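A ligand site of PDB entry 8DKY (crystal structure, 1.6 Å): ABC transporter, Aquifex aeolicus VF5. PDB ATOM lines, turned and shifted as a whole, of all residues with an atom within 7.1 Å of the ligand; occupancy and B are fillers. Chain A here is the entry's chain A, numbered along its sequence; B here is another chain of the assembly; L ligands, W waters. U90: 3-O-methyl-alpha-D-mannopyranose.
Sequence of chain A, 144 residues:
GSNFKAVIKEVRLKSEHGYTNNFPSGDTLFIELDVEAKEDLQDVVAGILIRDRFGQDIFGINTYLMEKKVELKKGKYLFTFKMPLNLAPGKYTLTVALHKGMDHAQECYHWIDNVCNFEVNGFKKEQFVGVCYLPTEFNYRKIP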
ATOM      1  N   VAL A  45     -14.211 -34.797   3.779  1.00  0.00           N
ATOM      2  CA  VAL A  45     -14.285 -33.340   3.752  1.00  0.00           C
ATOM      3  C   VAL A  45     -13.025 -32.828   3.082  1.00  0.00           C
ATOM      4  O   VAL A  45     -11.923 -33.332   3.333  1.00  0.00           O
ATOM      5  CB  VAL A  45     -14.433 -32.756   5.171  1.00  0.00           C
ATOM      6  CG1 VAL A  45     -14.454 -31.239   5.131  1.00  0.00           C
ATOM      7  CG2 VAL A  45     -15.689 -33.288   5.842  1.00  0.00           C
ATOM      8  N   ALA A  46     -13.192 -31.830   2.222  1.00  0.00           N
ATOM      9  CA  ALA A  46     -12.087 -31.155   1.547  1.00  0.00           C
ATOM     10  C   ALA A  46     -12.105 -29.683   1.922  1.00  0.00           C
ATOM     11  O   ALA A  46     -13.152 -29.028   1.863  1.00  0.00           O
ATOM     12  CB  ALA A  46     -12.191 -31.317   0.028  1.00  0.00           C
ATOM     13  N   GLY A  47     -10.947 -29.151   2.309  1.00  0.00           N
ATOM     14  CA  GLY A  47     -10.857 -27.799   2.815  1.00  0.00           C
ATOM     15  C   GLY A  47      -9.732 -27.005   2.171  1.00  0.00           C
ATOM     16  O   GLY A  47      -8.689 -27.542   1.822  1.00  0.00           O
ATOM     17  N   ILE A  48      -9.981 -25.694   2.044  1.00  0.00           N
ATOM     18  CA  ILE A  48      -9.014 -24.747   1.515  1.00  0.00           C
ATOM     19  C   ILE A  48      -8.866 -23.598   2.500  1.00  0.00           C
ATOM     20  O   ILE A  48      -9.796 -23.260   3.242  1.00  0.00           O
ATOM     21  CB  ILE A  48      -9.426 -24.213   0.122  1.00  0.00           C
ATOM     22  CG1 ILE A  48     -10.738 -23.444   0.226  1.00  0.00           C
ATOM     23  CG2 ILE A  48      -9.520 -25.343  -0.893  1.00  0.00           C
ATOM     24  CD1 ILE A  48     -10.824 -22.285  -0.734  1.00  0.00           C
ATOM     25  N   LEU A  49      -7.676 -22.982   2.482  1.00  0.00           N
ATOM     26  CA  LEU A  49      -7.346 -21.924   3.424  1.00  0.00           C
ATOM     27  C   LEU A  49      -6.362 -20.963   2.773  1.00  0.00           C
ATOM     28  O   LEU A  49      -5.212 -21.338   2.516  1.00  0.00           O
ATOM     29  CB  LEU A  49      -6.768 -22.506   4.706  1.00  0.00           C
ATOM     30  CG  LEU A  49      -6.274 -21.527   5.768  1.00  0.00           C
ATOM     31  CD1 LEU A  49      -7.417 -20.687   6.290  1.00  0.00           C
ATOM     32  CD2 LEU A  49      -5.614 -22.289   6.903  1.00  0.00           C
ATOM     33  N   ILE A  50      -6.805 -19.745   2.506  1.00  0.00           N
ATOM     34  CA  ILE A  50      -5.969 -18.682   1.961  1.00  0.00           C
ATOM     35  C   ILE A  50      -5.423 -17.849   3.113  1.00  0.00           C
ATOM     36  O   ILE A  50      -6.197 -17.339   3.939  1.00  0.00           O
ATOM     37  CB  ILE A  50      -6.769 -17.779   1.000  1.00  0.00           C
ATOM     38  CG1 ILE A  50      -7.252 -18.575  -0.213  1.00  0.00           C
ATOM     39  CG2 ILE A  50      -5.944 -16.575   0.584  1.00  0.00           C
ATOM     40  CD1 ILE A  50      -8.300 -17.821  -1.025  1.00  0.00           C
ATOM     41  N   PHE A  59      -9.049 -16.375   4.311  1.00  0.00           N
ATOM     42  CA  PHE A  59     -10.339 -17.023   4.077  1.00  0.00           C
ATOM     43  C   PHE A  59     -10.170 -18.531   3.995  1.00  0.00           C
ATOM     44  O   PHE A  59      -9.425 -19.008   3.145  1.00  0.00           O
ATOM     45  CB  PHE A  59     -11.016 -16.523   2.788  1.00  0.00           C
ATOM     46  CG  PHE A  59     -12.176 -17.375   2.365  1.00  0.00           C
ATOM     47  CD1 PHE A  59     -13.352 -17.394   3.112  1.00  0.00           C
ATOM     48  CD2 PHE A  59     -12.090 -18.191   1.251  1.00  0.00           C
ATOM     49  CE1 PHE A  59     -14.422 -18.184   2.726  1.00  0.00           C
ATOM     50  CE2 PHE A  59     -13.158 -18.992   0.865  1.00  0.00           C
ATOM     51  CZ  PHE A  59     -14.325 -18.988   1.610  1.00  0.00           C
ATOM     52  N   GLY A  60     -10.900 -19.262   4.816  1.00  0.00           N
ATOM     53  CA  GLY A  60     -10.872 -20.715   4.758  1.00  0.00           C
ATOM     54  C   GLY A  60     -12.271 -21.283   4.872  1.00  0.00           C
ATOM     55  O   GLY A  60     -13.126 -20.750   5.569  1.00  0.00           O
ATOM     56  N   ILE A  61     -12.484 -22.399   4.176  1.00  0.00           N
ATOM     57  CA  ILE A  61     -13.780 -23.059   4.170  1.00  0.00           C
ATOM     58  C   ILE A  61     -13.565 -24.515   3.764  1.00  0.00           C
ATOM     59  O   ILE A  61     -12.537 -24.860   3.185  1.00  0.00           O
ATOM     60  CB  ILE A  61     -14.768 -22.337   3.218  1.00  0.00           C
ATOM     61  CG1 ILE A  61     -16.228 -22.684   3.534  1.00  0.00           C
ATOM     62  CG2 ILE A  61     -14.448 -22.665   1.755  1.00  0.00           C
ATOM     63  CD1 ILE A  61     -17.242 -21.804   2.810  1.00  0.00           C
ATOM     64  N   ASN A  62     -14.535 -25.369   4.064  1.00  0.00           N
ATOM     65  CA  ASN A  62     -14.456 -26.761   3.646  1.00  0.00           C
ATOM     66  C   ASN A  62     -15.844 -27.258   3.250  1.00  0.00           C
ATOM     67  O   ASN A  62     -16.855 -26.575   3.438  1.00  0.00           O
ATOM     68  CB  ASN A  62     -13.787 -27.639   4.734  1.00  0.00           C
ATOM     69  CG  ASN A  62     -14.642 -27.836   5.977  1.00  0.00           C
ATOM     70  OD1 ASN A  62     -15.852 -28.034   5.909  1.00  0.00           O
ATOM     71  ND2 ASN A  62     -13.999 -27.781   7.140  1.00  0.00           N
ATOM     72  N   THR A  63     -15.876 -28.471   2.675  1.00  0.00           N
ATOM     73  CA  THR A  63     -17.098 -28.994   2.075  1.00  0.00           C
ATOM     74  C   THR A  63     -18.133 -29.397   3.124  1.00  0.00           C
ATOM     75  O   THR A  63     -19.312 -29.531   2.773  1.00  0.00           O
ATOM     76  CB  THR A  63     -16.770 -30.173   1.168  1.00  0.00           C
ATOM     77  OG1 THR A  63     -15.878 -31.061   1.844  1.00  0.00           O
ATOM     78  CG2 THR A  63     -16.099 -29.668  -0.122  1.00  0.00           C
ATOM     79  N   LEU A  65     -18.730 -27.393   5.791  1.00  0.00           N
ATOM     80  CA  LEU A  65     -19.371 -26.100   6.023  1.00  0.00           C
ATOM     81  C   LEU A  65     -20.246 -25.680   4.855  1.00  0.00           C
ATOM     82  O   LEU A  65     -21.216 -24.948   5.045  1.00  0.00           O
ATOM     83  CB  LEU A  65     -18.303 -25.052   6.308  1.00  0.00           C
ATOM     84  CG  LEU A  65     -17.400 -25.361   7.501  1.00  0.00           C
ATOM     85  CD1 LEU A  65     -16.390 -24.248   7.739  1.00  0.00           C
ATOM     86  CD2 LEU A  65     -18.251 -25.578   8.746  1.00  0.00           C
ATOM     87  N   THR A  95      -3.417 -23.339   1.481  1.00  0.00           N
ATOM     88  CA  THR A  95      -3.264 -24.563   2.247  1.00  0.00           C
ATOM     89  C   THR A  95      -4.482 -25.434   1.989  1.00  0.00           C
ATOM     90  O   THR A  95      -5.601 -24.929   1.902  1.00  0.00           O
ATOM     91  CB  THR A  95      -3.119 -24.252   3.738  1.00  0.00           C
ATOM     92  OG1 THR A  95      -1.862 -23.580   3.970  1.00  0.00           O
ATOM     93  CG2 THR A  95      -3.180 -25.511   4.587  1.00  0.00           C
ATOM     94  N   VAL A  96      -4.275 -26.746   1.840  1.00  0.00           N
ATOM     95  CA  VAL A  96      -5.369 -27.634   1.449  1.00  0.00           C
ATOM     96  C   VAL A  96      -5.393 -28.860   2.365  1.00  0.00           C
ATOM     97  O   VAL A  96      -4.400 -29.209   3.000  1.00  0.00           O
ATOM     98  CB  VAL A  96      -5.264 -28.078  -0.025  1.00  0.00           C
ATOM     99  CG1 VAL A  96      -5.453 -26.875  -0.953  1.00  0.00           C
ATOM    100  CG2 VAL A  96      -3.925 -28.753  -0.286  1.00  0.00           C
ATOM    101  N   ALA A  97      -6.560 -29.510   2.414  1.00  0.00           N
ATOM    102  CA  ALA A  97      -6.654 -30.682   3.284  1.00  0.00           C
ATOM    103  C   ALA A  97      -7.817 -31.584   2.894  1.00  0.00           C
ATOM    104  O   ALA A  97      -8.857 -31.128   2.406  1.00  0.00           O
ATOM    105  CB  ALA A  97      -6.810 -30.269   4.747  1.00  0.00           C
ATOM    106  N   LEU A  98      -7.613 -32.874   3.119  1.00  0.00           N
ATOM    107  CA  LEU A  98      -8.649 -33.902   3.116  1.00  0.00           C
ATOM    108  C   LEU A  98      -8.704 -34.520   4.497  1.00  0.00           C
ATOM    109  O   LEU A  98      -7.673 -34.964   5.020  1.00  0.00           O
ATOM    110  CB  LEU A  98      -8.362 -34.998   2.081  1.00  0.00           C
ATOM    111  CG  LEU A  98      -8.192 -34.608   0.620  1.00  0.00           C
ATOM    112  CD1 LEU A  98      -7.703 -35.817  -0.165  1.00  0.00           C
ATOM    113  CD2 LEU A  98      -9.495 -34.099   0.064  1.00  0.00           C
ATOM    114  N   HIS A  99      -9.890 -34.543   5.095  1.00  0.00           N
ATOM    115  CA  HIS A  99     -10.042 -35.071   6.448  1.00  0.00           C
ATOM    116  C   HIS A  99     -11.466 -35.575   6.643  1.00  0.00           C
ATOM    117  O   HIS A  99     -12.255 -35.631   5.701  1.00  0.00           O
ATOM    118  CB  HIS A  99      -9.642 -34.020   7.497  1.00  0.00           C
ATOM    119  CG  HIS A  99     -10.346 -32.711   7.337  1.00  0.00           C
ATOM    120  ND1 HIS A  99     -11.601 -32.469   7.841  1.00  0.00           N
ATOM    121  CD2 HIS A  99      -9.948 -31.556   6.744  1.00  0.00           C
ATOM    122  CE1 HIS A  99     -11.956 -31.224   7.564  1.00  0.00           C
ATOM    123  NE2 HIS A  99     -10.974 -30.654   6.898  1.00  0.00           N
ATOM    124  N   GLY A 101     -14.828 -35.107   9.332  1.00  0.00           N
ATOM    125  CA  GLY A 101     -15.352 -34.207  10.314  1.00  0.00           C
ATOM    126  C   GLY A 101     -15.102 -32.755   9.945  1.00  0.00           C
ATOM    127  O   GLY A 101     -14.162 -32.413   9.228  1.00  0.00           O
ATOM    128  N   MET A 102     -15.982 -31.894  10.471  1.00  0.00           N
ATOM    129  CA  MET A 102     -15.932 -30.477  10.169  1.00  0.00           C
ATOM    130  C   MET A 102     -14.608 -29.868  10.584  1.00  0.00           C
ATOM    131  O   MET A 102     -14.104 -28.966   9.899  1.00  0.00           O
ATOM    132  CB  MET A 102     -17.089 -29.759  10.858  1.00  0.00           C
ATOM    133  CG  MET A 102     -16.806 -29.311  12.301  1.00  0.00           C
ATOM    134  SD  MET A 102     -18.337 -28.706  13.037  1.00  0.00           S
ATOM    135  CE  MET A 102     -19.100 -28.202  11.514  1.00  0.00           C
ATOM    136  N   ASP A 103     -14.015 -30.329  11.685  1.00  0.00           N
ATOM    137  CA  ASP A 103     -12.902 -29.498  12.089  1.00  0.00           C
ATOM    138  C   ASP A 103     -11.631 -30.355  12.242  1.00  0.00           C
ATOM    139  O   ASP A 103     -10.684 -29.963  12.926  1.00  0.00           O
ATOM    140  CB  ASP A 103     -13.309 -28.684  13.326  1.00  0.00           C
ATOM    141  CG  ASP A 103     -12.297 -27.674  13.665  1.00  0.00           C
ATOM    142  OD1 ASP A 103     -12.271 -26.701  12.906  1.00  0.00           O
ATOM    143  OD2 ASP A 103     -11.578 -27.802  14.659  1.00  0.00           O
ATOM    144  N   HIS A 104     -11.598 -31.450  11.464  1.00  0.00           N
ATOM    145  CA  HIS A 104     -10.603 -32.546  11.384  1.00  0.00           C
ATOM    146  C   HIS A 104     -10.208 -33.138  12.740  1.00  0.00           C
ATOM    147  O   HIS A 104      -9.091 -33.625  12.925  1.00  0.00           O
ATOM    148  CB  HIS A 104      -9.332 -32.175  10.599  1.00  0.00           C
ATOM    149  CG  HIS A 104      -8.494 -31.093  11.224  1.00  0.00           C
ATOM    150  ND1 HIS A 104      -8.428 -29.813  10.714  1.00  0.00           N
ATOM    151  CD2 HIS A 104      -7.663 -31.120  12.293  1.00  0.00           C
ATOM    152  CE1 HIS A 104      -7.610 -29.093  11.463  1.00  0.00           C
ATOM    153  NE2 HIS A 104      -7.138 -29.867  12.429  1.00  0.00           N
ATOM    154  N   TRP A 111      -2.899 -33.242   4.856  1.00  0.00           N
ATOM    155  CA  TRP A 111      -2.849 -31.800   5.071  1.00  0.00           C
ATOM    156  C   TRP A 111      -1.590 -31.247   4.405  1.00  0.00           C
ATOM    157  O   TRP A 111      -0.496 -31.752   4.663  1.00  0.00           O
ATOM    158  CB  TRP A 111      -2.859 -31.468   6.568  1.00  0.00           C
ATOM    159  CG  TRP A 111      -2.840 -30.003   6.894  1.00  0.00           C
ATOM    160  CD1 TRP A 111      -1.778 -29.152   6.821  1.00  0.00           C
ATOM    161  CD2 TRP A 111      -3.950 -29.223   7.372  1.00  0.00           C
ATOM    162  NE1 TRP A 111      -2.158 -27.885   7.202  1.00  0.00           N
ATOM    163  CE2 TRP A 111      -3.480 -27.906   7.545  1.00  0.00           C
ATOM    164  CE3 TRP A 111      -5.286 -29.507   7.660  1.00  0.00           C
ATOM    165  CZ2 TRP A 111      -4.308 -26.876   7.999  1.00  0.00           C
ATOM    166  CZ3 TRP A 111      -6.106 -28.487   8.107  1.00  0.00           C
ATOM    167  CH2 TRP A 111      -5.611 -27.186   8.275  1.00  0.00           C
ATOM    168  N   ILE A 112      -1.753 -30.237   3.551  1.00  0.00           N
ATOM    169  CA  ILE A 112      -0.617 -29.607   2.872  1.00  0.00           C
ATOM    170  C   ILE A 112      -0.632 -28.119   3.196  1.00  0.00           C
ATOM    171  O   ILE A 112      -1.491 -27.373   2.688  1.00  0.00           O
ATOM    172  CB  ILE A 112      -0.648 -29.846   1.360  1.00  0.00           C
ATOM    173  CG1 ILE A 112      -0.755 -31.339   1.043  1.00  0.00           C
ATOM    174  CG2 ILE A 112       0.627 -29.296   0.736  1.00  0.00           C
ATOM    175  CD1 ILE A 112      -0.795 -31.638  -0.442  1.00  0.00           C
ATOM    176  N   GLN B 127     -20.552 -20.959   7.255  1.00  0.00           N
ATOM    177  CA  GLN B 127     -19.506 -20.666   8.217  1.00  0.00           C
ATOM    178  C   GLN B 127     -18.150 -20.679   7.515  1.00  0.00           C
ATOM    179  O   GLN B 127     -17.960 -21.353   6.501  1.00  0.00           O
ATOM    180  CB  GLN B 127     -19.541 -21.702   9.337  1.00  0.00           C
ATOM    181  CG  GLN B 127     -18.462 -21.568  10.398  1.00  0.00           C
ATOM    182  CD  GLN B 127     -18.603 -22.618  11.485  1.00  0.00           C
ATOM    183  OE1 GLN B 127     -17.617 -23.213  11.907  1.00  0.00           O
ATOM    184  NE2 GLN B 127     -19.829 -22.857  11.924  1.00  0.00           N
ATOM    185  N   PHE B 128     -17.203 -19.901   8.045  1.00  0.00           N
ATOM    186  CA  PHE B 128     -15.899 -19.786   7.417  1.00  0.00           C
ATOM    187  C   PHE B 128     -14.909 -19.243   8.436  1.00  0.00           C
ATOM    188  O   PHE B 128     -15.293 -18.679   9.460  1.00  0.00           O
ATOM    189  CB  PHE B 128     -15.943 -18.877   6.181  1.00  0.00           C
ATOM    190  CG  PHE B 128     -16.207 -17.438   6.511  1.00  0.00           C
ATOM    191  CD1 PHE B 128     -15.154 -16.547   6.682  1.00  0.00           C
ATOM    192  CD2 PHE B 128     -17.499 -16.976   6.683  1.00  0.00           C
ATOM    193  CE1 PHE B 128     -15.381 -15.224   6.994  1.00  0.00           C
ATOM    194  CE2 PHE B 128     -17.735 -15.645   7.001  1.00  0.00           C
ATOM    195  CZ  PHE B 128     -16.678 -14.774   7.161  1.00  0.00           C
ATOM    196  N   VAL B 129     -13.619 -19.419   8.138  1.00  0.00           N
ATOM    197  CA  VAL B 129     -12.548 -18.839   8.933  1.00  0.00           C
ATOM    198  C   VAL B 129     -11.866 -17.760   8.104  1.00  0.00           C
ATOM    199  O   VAL B 129     -11.951 -17.729   6.874  1.00  0.00           O
ATOM    200  CB  VAL B 129     -11.541 -19.894   9.424  1.00  0.00           C
ATOM    201  CG1 VAL B 129     -12.250 -21.028  10.152  1.00  0.00           C
ATOM    202  CG2 VAL B 129     -10.720 -20.423   8.266  1.00  0.00           C
HETATM  203  C1' U90 L   1     -10.422 -27.129   8.383  1.00  0.00           C
HETATM  204  C2' U90 L   1      -9.842 -27.232   7.025  1.00  0.00           C
HETATM  205  C3' U90 L   1      -9.477 -25.935   6.498  1.00  0.00           C
HETATM  206  C4' U90 L   1     -10.633 -25.026   6.432  1.00  0.00           C
HETATM  207  C5' U90 L   1     -11.258 -24.837   7.825  1.00  0.00           C
HETATM  208  C6' U90 L   1     -12.452 -24.104   7.718  1.00  0.00           C
HETATM  209  C7' U90 L   1      -7.517 -26.303   5.142  1.00  0.00           C
HETATM  210  O1' U90 L   1      -9.424 -26.680   9.246  1.00  0.00           O
HETATM  211  O2' U90 L   1     -10.861 -27.829   6.154  1.00  0.00           O
HETATM  212  O3' U90 L   1      -8.889 -26.076   5.158  1.00  0.00           O
HETATM  213  O4' U90 L   1     -10.136 -23.761   6.056  1.00  0.00           O
HETATM  214  O5' U90 L   1     -11.558 -26.196   8.435  1.00  0.00           O
HETATM  215  O6' U90 L   1     -12.981 -24.017   8.998  1.00  0.00           O
HETATM  216  O   HOH W   1     -14.189 -26.029  10.558  1.00  0.00           O
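Water W1 lies within hydrogen-bond range of O6' of the ligand (2.8 Å), O of Met 102 (3.0 Å) and OD1 of Asp 103 (3.1 Å).
O of Ile 61 sits at hydrogen-bond distance from N of Ile 48, 2.9 Å away. O of His 99 sits at hydrogen-bond distance from N of Val 45, at 2.9 Å. ND1 of His 99 lies within hydrogen-bond range of O of Gly 101. The side-chain amide oxygen (OD1) of Asn 62 lies within hydrogen-bond range of the backbone NH (N) of Leu 65, at 3.0 Å. The side-chain amide nitrogen (ND2) of Asn 62 lies within hydrogen-bond range of the backbone carbonyl oxygen (O) of Met 102, 3.0 Å away. N of Gly 47 lies within hydrogen-bond range of O of Ala 97. The backbone carbonyl oxygen (O) of Val 129 of chain B is in hydrogen-bond range of the backbone NH (N) of Gly 60 (2.8 Å). The backbone carbonyl oxygen of Leu 49 lies within hydrogen-bond range of the backbone NH of Thr 95.
The backbone NH (N) of Ile 48 lies within hydrogen-bond range of an oxygen (O3') of the ligand, at 3.3 Å. O of Ile 48 lies within hydrogen-bond range of O4' of the ligand (2.9 Å). A ring nitrogen (NE2) of His 99 lies within hydrogen-bond range of an oxygen (O2') of the ligand (2.9 Å). O5' of the ligand is in hydrogen-bond range of ND2 of Asn 62 (3.2 Å). The backbone NH (N) of Ile 61 lies within hydrogen-bond range of an oxygen (O4') of the ligand.
Gly 47 touches the ligand (C to O3', 3.2 Å). Leu 49 touches the ligand. CA of Gly 60 touches O4' of the ligand, 3.4 Å away. CD1 of Leu 65 touches O6' of the ligand (3.6 Å). His 104 touches the ligand (ND1 to O1', 3.6 Å). Trp 111 touches the ligand (CH2 to C7', 3.8 Å). Val 129 of chain B touches the ligand (CG1 to O6', 3.3 Å).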
